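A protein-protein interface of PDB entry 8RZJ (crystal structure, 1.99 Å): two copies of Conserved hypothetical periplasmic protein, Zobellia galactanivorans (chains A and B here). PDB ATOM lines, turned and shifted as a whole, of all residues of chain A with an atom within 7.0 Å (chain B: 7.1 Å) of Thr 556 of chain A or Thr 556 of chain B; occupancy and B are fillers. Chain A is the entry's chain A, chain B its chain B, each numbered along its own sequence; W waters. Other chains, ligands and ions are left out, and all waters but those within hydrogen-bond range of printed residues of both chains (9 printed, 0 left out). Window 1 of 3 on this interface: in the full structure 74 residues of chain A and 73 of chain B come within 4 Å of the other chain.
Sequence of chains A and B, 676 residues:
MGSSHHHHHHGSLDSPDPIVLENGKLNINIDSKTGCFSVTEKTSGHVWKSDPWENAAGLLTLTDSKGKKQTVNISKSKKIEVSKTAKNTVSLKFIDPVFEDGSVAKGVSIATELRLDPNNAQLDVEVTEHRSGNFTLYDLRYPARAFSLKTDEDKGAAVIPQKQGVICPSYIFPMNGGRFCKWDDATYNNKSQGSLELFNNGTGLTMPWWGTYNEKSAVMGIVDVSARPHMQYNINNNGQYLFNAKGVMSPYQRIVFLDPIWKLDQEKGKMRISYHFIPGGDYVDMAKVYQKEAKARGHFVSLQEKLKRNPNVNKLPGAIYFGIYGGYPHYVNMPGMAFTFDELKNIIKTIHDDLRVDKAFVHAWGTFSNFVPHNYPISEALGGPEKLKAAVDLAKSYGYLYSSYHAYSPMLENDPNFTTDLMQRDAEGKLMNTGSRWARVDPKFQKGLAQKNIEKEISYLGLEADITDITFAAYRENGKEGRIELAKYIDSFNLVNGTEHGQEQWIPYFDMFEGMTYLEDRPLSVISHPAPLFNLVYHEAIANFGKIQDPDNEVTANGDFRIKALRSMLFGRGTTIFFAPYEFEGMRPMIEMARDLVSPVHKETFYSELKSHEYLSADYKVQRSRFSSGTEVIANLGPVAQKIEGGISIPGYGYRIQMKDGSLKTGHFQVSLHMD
The backbone carbonyl oxygen (O) of Thr 556 of chain B sits close to the backbone carbonyl oxygen (O) of Thr 556 of chain A, 3.5 Å away.
The guanidinium group (NE) of Arg 179 of chain A is in salt-bridge range of the side-chain carboxylate (OE1) of Glu 554 of chain B.
NH2 of Arg 179 of chain A is in hydrogen-bond range of O of Val 555 of chain B, 2.8 Å away.
The side-chain carboxylate of Glu 554 of chain A lies within salt-bridge range of the guanidinium group of Arg 179 of chain B, at 2.8 Å.
OE2 of Glu 520 of chain A lies within salt-bridge range of NZ of Lys 182 of chain B, at 2.8 Å.
The guanidinium group (NH2) of Arg 179 of chain B sits at hydrogen-bond distance from the backbone carbonyl oxygen (O) of Val 555 of chain A, at 2.8 Å.
NZ of Lys 182 of chain A is in salt-bridge range of OE2 of Glu 520 of chain B, at 2.7 Å.
The side-chain hydroxyl of Thr 556 of chain A lies close to the backbone NH of Asn 558 of chain A.
The side-chain amino group (NZ) of Lys 564 of chain A sits at hydrogen-bond distance from the backbone carbonyl oxygen (O) of Glu 554 of chain A, 2.8 Å away.
The side-chain hydroxyl of Thr 556 of chain A sits at hydrogen-bond distance from the side-chain amino group of Lys 564 of chain A (3.4 Å).
OG1 of Thr 556 of chain B is in hydrogen-bond range of NZ of Lys 564 of chain B (3.3 Å).
The backbone carbonyl oxygen (O) of Glu 554 of chain B lies within hydrogen-bond range of the side-chain amino group (NZ) of Lys 564 of chain B (2.9 Å).
OD1 of Asp 560 of chain B lies within hydrogen-bond range of N of Ile 563 of chain B, at 3.1 Å.
Among the printed residues, merely in contact across the chains: Lys 182 of chain A with Gln 549 of chain B, Gln 549 of chain A with Lys 182 of chain B, Asp 560 of chain A with Val 555 of chain B, Ala 557 of chain A with Ala 557 of chain B, Val 555 of chain A with Asp 560 of chain B, Arg 179 of chain A with Thr 556 of chain B, Thr 556 of chain A with Arg 179 of chain B, Gly 559 of chain A with Val 555 of chain B, Val 555 of chain A with Gly 559 of chain B, Val 555 of chain A with Val 555 of chain B, Thr 556 of chain A with Ala 557 of chain B and Ala 557 of chain A with Thr 556 of chain B.
Of the printed residues of chain B, Thr 556 of chain A touches Arg 179, Thr 556 and Ala 557.
Printed residues of chain B within 4 Å of Ala 557 of chain A: Thr 556 and Ala 557.
Asn 558 of chain A touches none of the printed residues of chain B.
Of the printed residues of chain B, Gly 559 of chain A touches Val 555.
Printed residues of chain A within 4 Å of Arg 179 of chain B: Glu 554 (2.8 Å), Val 555 (2.8 Å) and Thr 556 (3.7 Å).
Of the printed residues of chain A, Glu 520 of chain B touches Lys 182.
Thr 556 of chain B touches just these residues of chain A: Arg 179 (3.7 Å), Thr 556 (3.5 Å) and Ala 557 (3.9 Å).
Lys 564 of chain B touches none of the printed residues of chain A.
Hydrophobic or aromatic side chains of chain B that line the printed part of chain A: Val 555.
Of the 15 printed residues of chain A, 10 touch a printed residue of chain B.
Hydrophobic or aromatic side chains of chain A within 4 Å of the printed part of chain B: Val 555.
Among the printed residues, Asp or Glu carboxylates within 4 Å of a Lys or Arg side-chain nitrogen of the other chain: Arg 179 of chain A with Glu 554 of chain B, Lys 182 of chain A with Glu 520 of chain B, Glu 520 of chain A with Lys 182 of chain B and Glu 554 of chain A with Arg 179 of chain B.
Val 555 of chain A touches Gly 559 of chain B, and with the chains exchanged Gly 559 of chain A touches Val 555 of chain B.
Val 555 of chain A touches Asp 560 of chain B, and with the chains exchanged Asp 560 of chain A touches Val 555 of chain B.
Thr 556 of chain A touches its own counterpart, Thr 556 of chain B.
Thr 556 of chain A touches Ala 557 of chain B, and with the chains exchanged Ala 557 of chain A touches Thr 556 of chain B.
Of the 19 pairs that touch across the chains among the printed residues, 19 have their exchanged pair printed and touching as well.
Water W1 bridges the side-chain carboxylate (OD2) of Asp 560 of chain B (2.6 Å) and the side-chain carboxylate (OD2) of Asp 560 of chain A (2.6 Å).
Water W3 lies within hydrogen-bond range of O of Gln 549 of chain A, NZ of Lys 182 of chain B and NE of Arg 179 of chain B.
Water W4 bridges the side-chain carboxylate of Glu 520 of chain B (2.6 Å) and the side-chain amino group of Lys 182 of chain A (2.9 Å).
Water W2 lies within hydrogen-bond range of O of Gln 549 of chain B (2.7 Å), NZ of Lys 182 of chain A (2.8 Å) and NE of Arg 179 of chain A (3.2 Å).
Water W9 lies within hydrogen-bond range of N of Val 555 of chain B (2.8 Å), OE1 of Glu 554 of chain B (2.9 Å) and NH2 of Arg 179 of chain A (3.5 Å).
Water W7 bridges OE1 of Glu 554 of chain B (3.3 Å) and NE of Arg 179 of chain A (3.5 Å).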
ATOM      1  N   ARG A 179     -22.746  29.771  -3.097  1.00  0.00           N
ATOM      2  CA  ARG A 179     -23.410  31.042  -2.832  1.00  0.00           C
ATOM      3  C   ARG A 179     -24.229  31.489  -4.034  1.00  0.00           C
ATOM      4  O   ARG A 179     -25.385  31.907  -3.892  1.00  0.00           O
ATOM      5  CB  ARG A 179     -22.370  32.103  -2.472  1.00  0.00           C
ATOM      6  CG  ARG A 179     -21.455  31.694  -1.339  1.00  0.00           C
ATOM      7  CD  ARG A 179     -22.233  31.682  -0.033  1.00  0.00           C
ATOM      8  NE  ARG A 179     -21.399  31.345   1.111  1.00  0.00           N
ATOM      9  CZ  ARG A 179     -21.854  31.252   2.357  1.00  0.00           C
ATOM     10  NH1 ARG A 179     -23.142  31.485   2.619  1.00  0.00           N
ATOM     11  NH2 ARG A 179     -21.028  30.932   3.343  1.00  0.00           N
ATOM     12  N   LYS A 182     -27.584  29.695  -4.345  1.00  0.00           N
ATOM     13  CA  LYS A 182     -28.553  30.141  -3.344  1.00  0.00           C
ATOM     14  C   LYS A 182     -28.998  31.584  -3.603  1.00  0.00           C
ATOM     15  O   LYS A 182     -30.181  31.918  -3.445  1.00  0.00           O
ATOM     16  CB  LYS A 182     -27.965  30.013  -1.935  1.00  0.00           C
ATOM     17  CG  LYS A 182     -27.700  28.573  -1.460  1.00  0.00           C
ATOM     18  CD  LYS A 182     -27.160  28.578  -0.042  1.00  0.00           C
ATOM     19  CE  LYS A 182     -25.684  28.942  -0.015  1.00  0.00           C
ATOM     20  NZ  LYS A 182     -25.122  28.951   1.366  1.00  0.00           N
ATOM     21  N   GLU A 520     -27.777  35.144  12.719  1.00  0.00           N
ATOM     22  CA  GLU A 520     -27.242  34.070  11.885  1.00  0.00           C
ATOM     23  C   GLU A 520     -28.229  33.694  10.784  1.00  0.00           C
ATOM     24  O   GLU A 520     -27.884  33.684   9.597  1.00  0.00           O
ATOM     25  CB  GLU A 520     -26.884  32.855  12.754  1.00  0.00           C
ATOM     26  CG  GLU A 520     -25.758  33.140  13.743  1.00  0.00           C
ATOM     27  CD  GLU A 520     -25.684  32.122  14.866  1.00  0.00           C
ATOM     28  OE1 GLU A 520     -25.586  30.912  14.555  1.00  0.00           O
ATOM     29  OE2 GLU A 520     -25.733  32.535  16.055  1.00  0.00           O
ATOM     30  N   GLN A 549     -24.186  35.296  21.367  1.00  0.00           N
ATOM     31  CA  GLN A 549     -24.632  34.031  20.778  1.00  0.00           C
ATOM     32  C   GLN A 549     -23.869  33.671  19.512  1.00  0.00           C
ATOM     33  O   GLN A 549     -23.931  32.516  19.074  1.00  0.00           O
ATOM     34  CB  GLN A 549     -26.125  34.058  20.432  1.00  0.00           C
ATOM     35  CG  GLN A 549     -27.080  34.053  21.617  1.00  0.00           C
ATOM     36  CD  GLN A 549     -27.541  35.448  22.003  1.00  0.00           C
ATOM     37  OE1 GLN A 549     -26.816  36.429  21.812  1.00  0.00           O
ATOM     38  NE2 GLN A 549     -28.756  35.546  22.543  1.00  0.00           N
ATOM     39  N   ASP A 550     -23.188  34.635  18.902  1.00  0.00           N
ATOM     40  CA  ASP A 550     -22.475  34.435  17.642  1.00  0.00           C
ATOM     41  C   ASP A 550     -21.073  35.020  17.770  1.00  0.00           C
ATOM     42  O   ASP A 550     -20.657  35.877  16.984  1.00  0.00           O
ATOM     43  CB  ASP A 550     -23.250  35.087  16.501  1.00  0.00           C
ATOM     44  CG  ASP A 550     -22.625  34.834  15.153  1.00  0.00           C
ATOM     45  OD1 ASP A 550     -21.874  33.839  15.027  1.00  0.00           O
ATOM     46  OD2 ASP A 550     -22.862  35.647  14.226  1.00  0.00           O
ATOM     47  N   PRO A 551     -20.316  34.587  18.766  1.00  0.00           N
ATOM     48  CA  PRO A 551     -19.049  35.251  19.073  1.00  0.00           C
ATOM     49  C   PRO A 551     -17.983  34.859  18.057  1.00  0.00           C
ATOM     50  O   PRO A 551     -18.187  34.000  17.201  1.00  0.00           O
ATOM     51  CB  PRO A 551     -18.724  34.707  20.463  1.00  0.00           C
ATOM     52  CG  PRO A 551     -19.186  33.273  20.356  1.00  0.00           C
ATOM     53  CD  PRO A 551     -20.460  33.329  19.521  1.00  0.00           C
ATOM     54  N   GLU A 554     -16.898  31.100  17.625  1.00  0.00           N
ATOM     55  CA  GLU A 554     -17.822  30.094  17.111  1.00  0.00           C
ATOM     56  C   GLU A 554     -17.918  30.208  15.595  1.00  0.00           C
ATOM     57  O   GLU A 554     -17.845  31.307  15.042  1.00  0.00           O
ATOM     58  CB  GLU A 554     -19.214  30.238  17.740  1.00  0.00           C
ATOM     59  CG  GLU A 554     -19.312  29.661  19.140  1.00  0.00           C
ATOM     60  CD  GLU A 554     -19.209  28.154  19.124  1.00  0.00           C
ATOM     61  OE1 GLU A 554     -20.000  27.522  18.395  1.00  0.00           O
ATOM     62  OE2 GLU A 554     -18.321  27.601  19.802  1.00  0.00           O
ATOM     63  N   VAL A 555     -18.071  29.068  14.927  1.00  0.00           N
ATOM     64  CA  VAL A 555     -18.198  29.011  13.474  1.00  0.00           C
ATOM     65  C   VAL A 555     -19.685  28.965  13.143  1.00  0.00           C
ATOM     66  O   VAL A 555     -20.396  28.054  13.579  1.00  0.00           O
ATOM     67  CB  VAL A 555     -17.465  27.791  12.899  1.00  0.00           C
ATOM     68  CG1 VAL A 555     -17.588  27.765  11.388  1.00  0.00           C
ATOM     69  CG2 VAL A 555     -15.991  27.789  13.335  1.00  0.00           C
ATOM     70  N   THR A 556     -20.178  29.965  12.411  1.00  0.00           N
ATOM     71  CA  THR A 556     -21.610  30.106  12.180  1.00  0.00           C
ATOM     72  C   THR A 556     -21.857  30.578  10.756  1.00  0.00           C
ATOM     73  O   THR A 556     -20.931  30.732   9.955  1.00  0.00           O
ATOM     74  CB  THR A 556     -22.257  31.102  13.153  1.00  0.00           C
ATOM     75  OG1 THR A 556     -21.838  32.441  12.831  1.00  0.00           O
ATOM     76  CG2 THR A 556     -21.898  30.776  14.592  1.00  0.00           C
ATOM     77  N   ALA A 557     -23.138  30.824  10.453  1.00  0.00           N
ATOM     78  CA  ALA A 557     -23.502  31.380   9.156  1.00  0.00           C
ATOM     79  C   ALA A 557     -22.764  32.678   8.877  1.00  0.00           C
ATOM     80  O   ALA A 557     -22.537  33.018   7.713  1.00  0.00           O
ATOM     81  CB  ALA A 557     -25.016  31.613   9.082  1.00  0.00           C
ATOM     82  N   ASN A 558     -22.375  33.409   9.919  1.00  0.00           N
ATOM     83  CA  ASN A 558     -21.672  34.674   9.754  1.00  0.00           C
ATOM     84  C   ASN A 558     -20.154  34.520   9.718  1.00  0.00           C
ATOM     85  O   ASN A 558     -19.447  35.523   9.629  1.00  0.00           O
ATOM     86  CB  ASN A 558     -22.080  35.643  10.863  1.00  0.00           C
ATOM     87  CG  ASN A 558     -23.538  36.074  10.739  1.00  0.00           C
ATOM     88  OD1 ASN A 558     -24.048  36.263   9.635  1.00  0.00           O
ATOM     89  ND2 ASN A 558     -24.211  36.213  11.864  1.00  0.00           N
ATOM     90  N   GLY A 559     -19.635  33.300   9.776  1.00  0.00           N
ATOM     91  CA  GLY A 559     -18.238  33.059   9.495  1.00  0.00           C
ATOM     92  C   GLY A 559     -17.543  32.359  10.638  1.00  0.00           C
ATOM     93  O   GLY A 559     -18.127  32.062  11.678  1.00  0.00           O
ATOM     94  N   ASP A 560     -16.268  32.077  10.415  1.00  0.00           N
ATOM     95  CA  ASP A 560     -15.378  31.558  11.429  1.00  0.00           C
ATOM     96  C   ASP A 560     -14.554  32.721  11.987  1.00  0.00           C
ATOM     97  O   ASP A 560     -14.855  33.890  11.736  1.00  0.00           O
ATOM     98  CB  ASP A 560     -14.517  30.449  10.822  1.00  0.00           C
ATOM     99  CG  ASP A 560     -13.676  30.936   9.653  1.00  0.00           C
ATOM    100  OD1 ASP A 560     -13.671  32.155   9.372  1.00  0.00           O
ATOM    101  OD2 ASP A 560     -13.007  30.095   9.007  1.00  0.00           O
ATOM    102  N   ILE A 563     -12.954  35.106   9.127  1.00  0.00           N
ATOM    103  CA  ILE A 563     -13.886  36.063   8.535  1.00  0.00           C
ATOM    104  C   ILE A 563     -14.304  37.119   9.559  1.00  0.00           C
ATOM    105  O   ILE A 563     -14.344  38.323   9.257  1.00  0.00           O
ATOM    106  CB  ILE A 563     -15.105  35.314   7.956  1.00  0.00           C
ATOM    107  CG1 ILE A 563     -14.691  34.457   6.760  1.00  0.00           C
ATOM    108  CG2 ILE A 563     -16.215  36.292   7.568  1.00  0.00           C
ATOM    109  CD1 ILE A 563     -15.702  33.366   6.370  1.00  0.00           C
ATOM    110  N   LYS A 564     -14.608  36.695  10.789  1.00  0.00           N
ATOM    111  CA  LYS A 564     -15.148  37.638  11.762  1.00  0.00           C
ATOM    112  C   LYS A 564     -14.085  38.630  12.231  1.00  0.00           C
ATOM    113  O   LYS A 564     -14.389  39.807  12.427  1.00  0.00           O
ATOM    114  CB  LYS A 564     -15.767  36.885  12.945  1.00  0.00           C
ATOM    115  CG  LYS A 564     -17.062  36.159  12.593  1.00  0.00           C
ATOM    116  CD  LYS A 564     -17.534  35.301  13.763  1.00  0.00           C
ATOM    117  CE  LYS A 564     -18.917  34.738  13.524  1.00  0.00           C
ATOM    118  NZ  LYS A 564     -19.198  33.670  14.544  1.00  0.00           N
ATOM    119  N   ARG B 179     -23.931  28.831  22.081  1.00  0.00           N
ATOM    120  CA  ARG B 179     -24.828  27.741  21.715  1.00  0.00           C
ATOM    121  C   ARG B 179     -25.805  27.435  22.838  1.00  0.00           C
ATOM    122  O   ARG B 179     -26.976  27.131  22.588  1.00  0.00           O
ATOM    123  CB  ARG B 179     -24.029  26.480  21.374  1.00  0.00           C
ATOM    124  CG  ARG B 179     -22.998  26.653  20.292  1.00  0.00           C
ATOM    125  CD  ARG B 179     -23.647  26.742  18.931  1.00  0.00           C
ATOM    126  NE  ARG B 179     -22.640  26.930  17.898  1.00  0.00           N
ATOM    127  CZ  ARG B 179     -22.913  27.105  16.612  1.00  0.00           C
ATOM    128  NH1 ARG B 179     -24.175  27.119  16.198  1.00  0.00           N
ATOM    129  NH2 ARG B 179     -21.920  27.270  15.743  1.00  0.00           N
ATOM    130  N   LYS B 182     -28.780  29.927  22.956  1.00  0.00           N
ATOM    131  CA  LYS B 182     -29.737  29.677  21.877  1.00  0.00           C
ATOM    132  C   LYS B 182     -30.498  28.372  22.097  1.00  0.00           C
ATOM    133  O   LYS B 182     -31.710  28.300  21.857  1.00  0.00           O
ATOM    134  CB  LYS B 182     -29.017  29.649  20.525  1.00  0.00           C
ATOM    135  CG  LYS B 182     -28.469  31.015  20.048  1.00  0.00           C
ATOM    136  CD  LYS B 182     -27.881  30.935  18.641  1.00  0.00           C
ATOM    137  CE  LYS B 182     -26.537  30.240  18.672  1.00  0.00           C
ATOM    138  NZ  LYS B 182     -25.903  30.089  17.341  1.00  0.00           N
ATOM    139  N   GLU B 520     -28.517  24.479   5.817  1.00  0.00           N
ATOM    140  CA  GLU B 520     -27.865  25.454   6.682  1.00  0.00           C
ATOM    141  C   GLU B 520     -28.866  26.085   7.649  1.00  0.00           C
ATOM    142  O   GLU B 520     -28.650  26.085   8.864  1.00  0.00           O
ATOM    143  CB  GLU B 520     -27.163  26.521   5.829  1.00  0.00           C
ATOM    144  CG  GLU B 520     -26.069  25.966   4.918  1.00  0.00           C
ATOM    145  CD  GLU B 520     -25.665  26.974   3.858  1.00  0.00           C
ATOM    146  OE1 GLU B 520     -25.277  28.101   4.236  1.00  0.00           O
ATOM    147  OE2 GLU B 520     -25.773  26.651   2.656  1.00  0.00           O
ATOM    148  N   GLN B 549     -24.390  23.458  -2.535  1.00  0.00           N
ATOM    149  CA  GLN B 549     -24.614  24.791  -1.972  1.00  0.00           C
ATOM    150  C   GLN B 549     -23.907  24.993  -0.637  1.00  0.00           C
ATOM    151  O   GLN B 549     -23.722  26.138  -0.209  1.00  0.00           O
ATOM    152  CB  GLN B 549     -26.103  25.081  -1.775  1.00  0.00           C
ATOM    153  CG  GLN B 549     -26.855  25.339  -3.057  1.00  0.00           C
ATOM    154  CD  GLN B 549     -27.671  24.138  -3.455  1.00  0.00           C
ATOM    155  OE1 GLN B 549     -27.263  22.992  -3.227  1.00  0.00           O
ATOM    156  NE2 GLN B 549     -28.842  24.382  -4.027  1.00  0.00           N
ATOM    157  N   ASP B 550     -23.500  23.913   0.021  1.00  0.00           N
ATOM    158  CA  ASP B 550     -22.841  23.978   1.324  1.00  0.00           C
ATOM    159  C   ASP B 550     -21.594  23.095   1.309  1.00  0.00           C
ATOM    160  O   ASP B 550     -21.472  22.141   2.088  1.00  0.00           O
ATOM    161  CB  ASP B 550     -23.819  23.543   2.412  1.00  0.00           C
ATOM    162  CG  ASP B 550     -23.243  23.675   3.797  1.00  0.00           C
ATOM    163  OD1 ASP B 550     -22.333  24.504   3.988  1.00  0.00           O
ATOM    164  OD2 ASP B 550     -23.693  22.935   4.698  1.00  0.00           O
ATOM    165  N   PRO B 551     -20.645  23.384   0.424  1.00  0.00           N
ATOM    166  CA  PRO B 551     -19.534  22.457   0.200  1.00  0.00           C
ATOM    167  C   PRO B 551     -18.444  22.633   1.251  1.00  0.00           C
ATOM    168  O   PRO B 551     -18.445  23.563   2.057  1.00  0.00           O
ATOM    169  CB  PRO B 551     -19.042  22.867  -1.185  1.00  0.00           C
ATOM    170  CG  PRO B 551     -19.179  24.391  -1.128  1.00  0.00           C
ATOM    171  CD  PRO B 551     -20.530  24.580  -0.436  1.00  0.00           C
ATOM    172  N   GLU B 554     -16.714  26.065   1.851  1.00  0.00           N
ATOM    173  CA  GLU B 554     -17.446  27.244   2.297  1.00  0.00           C
ATOM    174  C   GLU B 554     -17.608  27.217   3.814  1.00  0.00           C
ATOM    175  O   GLU B 554     -17.685  26.147   4.419  1.00  0.00           O
ATOM    176  CB  GLU B 554     -18.817  27.323   1.609  1.00  0.00           C
ATOM    177  CG  GLU B 554     -18.746  27.852   0.181  1.00  0.00           C
ATOM    178  CD  GLU B 554     -18.395  29.332   0.134  1.00  0.00           C
ATOM    179  OE1 GLU B 554     -19.104  30.129   0.786  1.00  0.00           O
ATOM    180  OE2 GLU B 554     -17.403  29.702  -0.537  1.00  0.00           O
ATOM    181  N   VAL B 555     -17.633  28.395   4.432  1.00  0.00           N
ATOM    182  CA  VAL B 555     -17.876  28.513   5.871  1.00  0.00           C
ATOM    183  C   VAL B 555     -19.344  28.873   6.081  1.00  0.00           C
ATOM    184  O   VAL B 555     -19.809  29.909   5.596  1.00  0.00           O
ATOM    185  CB  VAL B 555     -16.955  29.555   6.523  1.00  0.00           C
ATOM    186  CG1 VAL B 555     -17.210  29.601   8.023  1.00  0.00           C
ATOM    187  CG2 VAL B 555     -15.490  29.228   6.225  1.00  0.00           C
ATOM    188  N   THR B 556     -20.080  28.020   6.798  1.00  0.00           N
ATOM    189  CA  THR B 556     -21.534  28.137   6.903  1.00  0.00           C
ATOM    190  C   THR B 556     -21.979  27.730   8.300  1.00  0.00           C
ATOM    191  O   THR B 556     -21.172  27.345   9.153  1.00  0.00           O
ATOM    192  CB  THR B 556     -22.283  27.250   5.890  1.00  0.00           C
ATOM    193  OG1 THR B 556     -22.058  25.860   6.197  1.00  0.00           O
ATOM    194  CG2 THR B 556     -21.837  27.526   4.463  1.00  0.00           C
ATOM    195  N   ALA B 557     -23.297  27.770   8.506  1.00  0.00           N
ATOM    196  CA  ALA B 557     -23.856  27.299   9.764  1.00  0.00           C
ATOM    197  C   ALA B 557     -23.403  25.868  10.079  1.00  0.00           C
ATOM    198  O   ALA B 557     -23.297  25.496  11.249  1.00  0.00           O
ATOM    199  CB  ALA B 557     -25.385  27.398   9.725  1.00  0.00           C
ATOM    200  N   ASN B 558     -23.076  25.074   9.063  1.00  0.00           N
ATOM    201  CA  ASN B 558     -22.674  23.685   9.291  1.00  0.00           C
ATOM    202  C   ASN B 558     -21.173  23.505   9.465  1.00  0.00           C
ATOM    203  O   ASN B 558     -20.720  22.366   9.633  1.00  0.00           O
ATOM    204  CB  ASN B 558     -23.189  22.805   8.156  1.00  0.00           C
ATOM    205  CG  ASN B 558     -24.695  22.725   8.162  1.00  0.00           C
ATOM    206  OD1 ASN B 558     -25.304  22.681   9.229  1.00  0.00           O
ATOM    207  ND2 ASN B 558     -25.309  22.736   6.984  1.00  0.00           N
ATOM    208  N   GLY B 559     -20.407  24.586   9.453  1.00  0.00           N
ATOM    209  CA  GLY B 559     -19.015  24.565   9.847  1.00  0.00           C
ATOM    210  C   GLY B 559     -18.089  25.036   8.741  1.00  0.00           C
ATOM    211  O   GLY B 559     -18.510  25.401   7.645  1.00  0.00           O
ATOM    212  N   ASP B 560     -16.801  25.042   9.072  1.00  0.00           N
ATOM    213  CA  ASP B 560     -15.720  25.361   8.160  1.00  0.00           C
ATOM    214  C   ASP B 560     -15.098  24.055   7.663  1.00  0.00           C
ATOM    215  O   ASP B 560     -15.653  22.967   7.853  1.00  0.00           O
ATOM    216  CB  ASP B 560     -14.690  26.256   8.860  1.00  0.00           C
ATOM    217  CG  ASP B 560     -14.143  25.631  10.144  1.00  0.00           C
ATOM    218  OD1 ASP B 560     -14.502  24.484  10.486  1.00  0.00           O
ATOM    219  OD2 ASP B 560     -13.353  26.301  10.834  1.00  0.00           O
ATOM    220  N   ILE B 563     -14.364  21.396  10.598  1.00  0.00           N
ATOM    221  CA  ILE B 563     -15.519  20.671  11.094  1.00  0.00           C
ATOM    222  C   ILE B 563     -16.048  19.730  10.027  1.00  0.00           C
ATOM    223  O   ILE B 563     -16.362  18.566  10.306  1.00  0.00           O
ATOM    224  CB  ILE B 563     -16.601  21.668  11.560  1.00  0.00           C
ATOM    225  CG1 ILE B 563     -16.116  22.447  12.788  1.00  0.00           C
ATOM    226  CG2 ILE B 563     -17.905  20.939  11.840  1.00  0.00           C
ATOM    227  CD1 ILE B 563     -16.903  23.741  13.064  1.00  0.00           C
ATOM    228  N   LYS B 564     -16.148  20.206   8.785  1.00  0.00           N
ATOM    229  CA  LYS B 564     -16.777  19.383   7.760  1.00  0.00           C
ATOM    230  C   LYS B 564     -15.910  18.184   7.400  1.00  0.00           C
ATOM    231  O   LYS B 564     -16.427  17.086   7.157  1.00  0.00           O
ATOM    232  CB  LYS B 564     -17.093  20.228   6.523  1.00  0.00           C
ATOM    233  CG  LYS B 564     -18.354  21.088   6.698  1.00  0.00           C
ATOM    234  CD  LYS B 564     -18.389  22.212   5.653  1.00  0.00           C
ATOM    235  CE  LYS B 564     -19.682  23.043   5.754  1.00  0.00           C
ATOM    236  NZ  LYS B 564     -19.751  24.083   4.681  1.00  0.00           N
HETATM  237  O   HOH W   1     -11.640  28.111  10.107  1.00  0.00           O
HETATM  238  O   HOH W   2     -22.438  28.302   0.755  1.00  0.00           O
HETATM  239  O   HOH W   3     -23.014  30.221  18.270  1.00  0.00           O
HETATM  240  O   HOH W   4     -26.798  30.129   3.466  1.00  0.00           O
HETATM  241  O   HOH W   5     -27.480  29.168  15.201  1.00  0.00           O
HETATM  242  O   HOH W   6     -20.438  25.358  12.663  1.00  0.00           O
HETATM  243  O   HOH W   7     -18.727  33.312   0.044  1.00  0.00           O
HETATM  244  O   HOH W   8     -19.710  32.430   6.528  1.00  0.00           O
HETATM  245  O   HOH W   9     -17.560  30.864   3.128  1.00  0.00           O
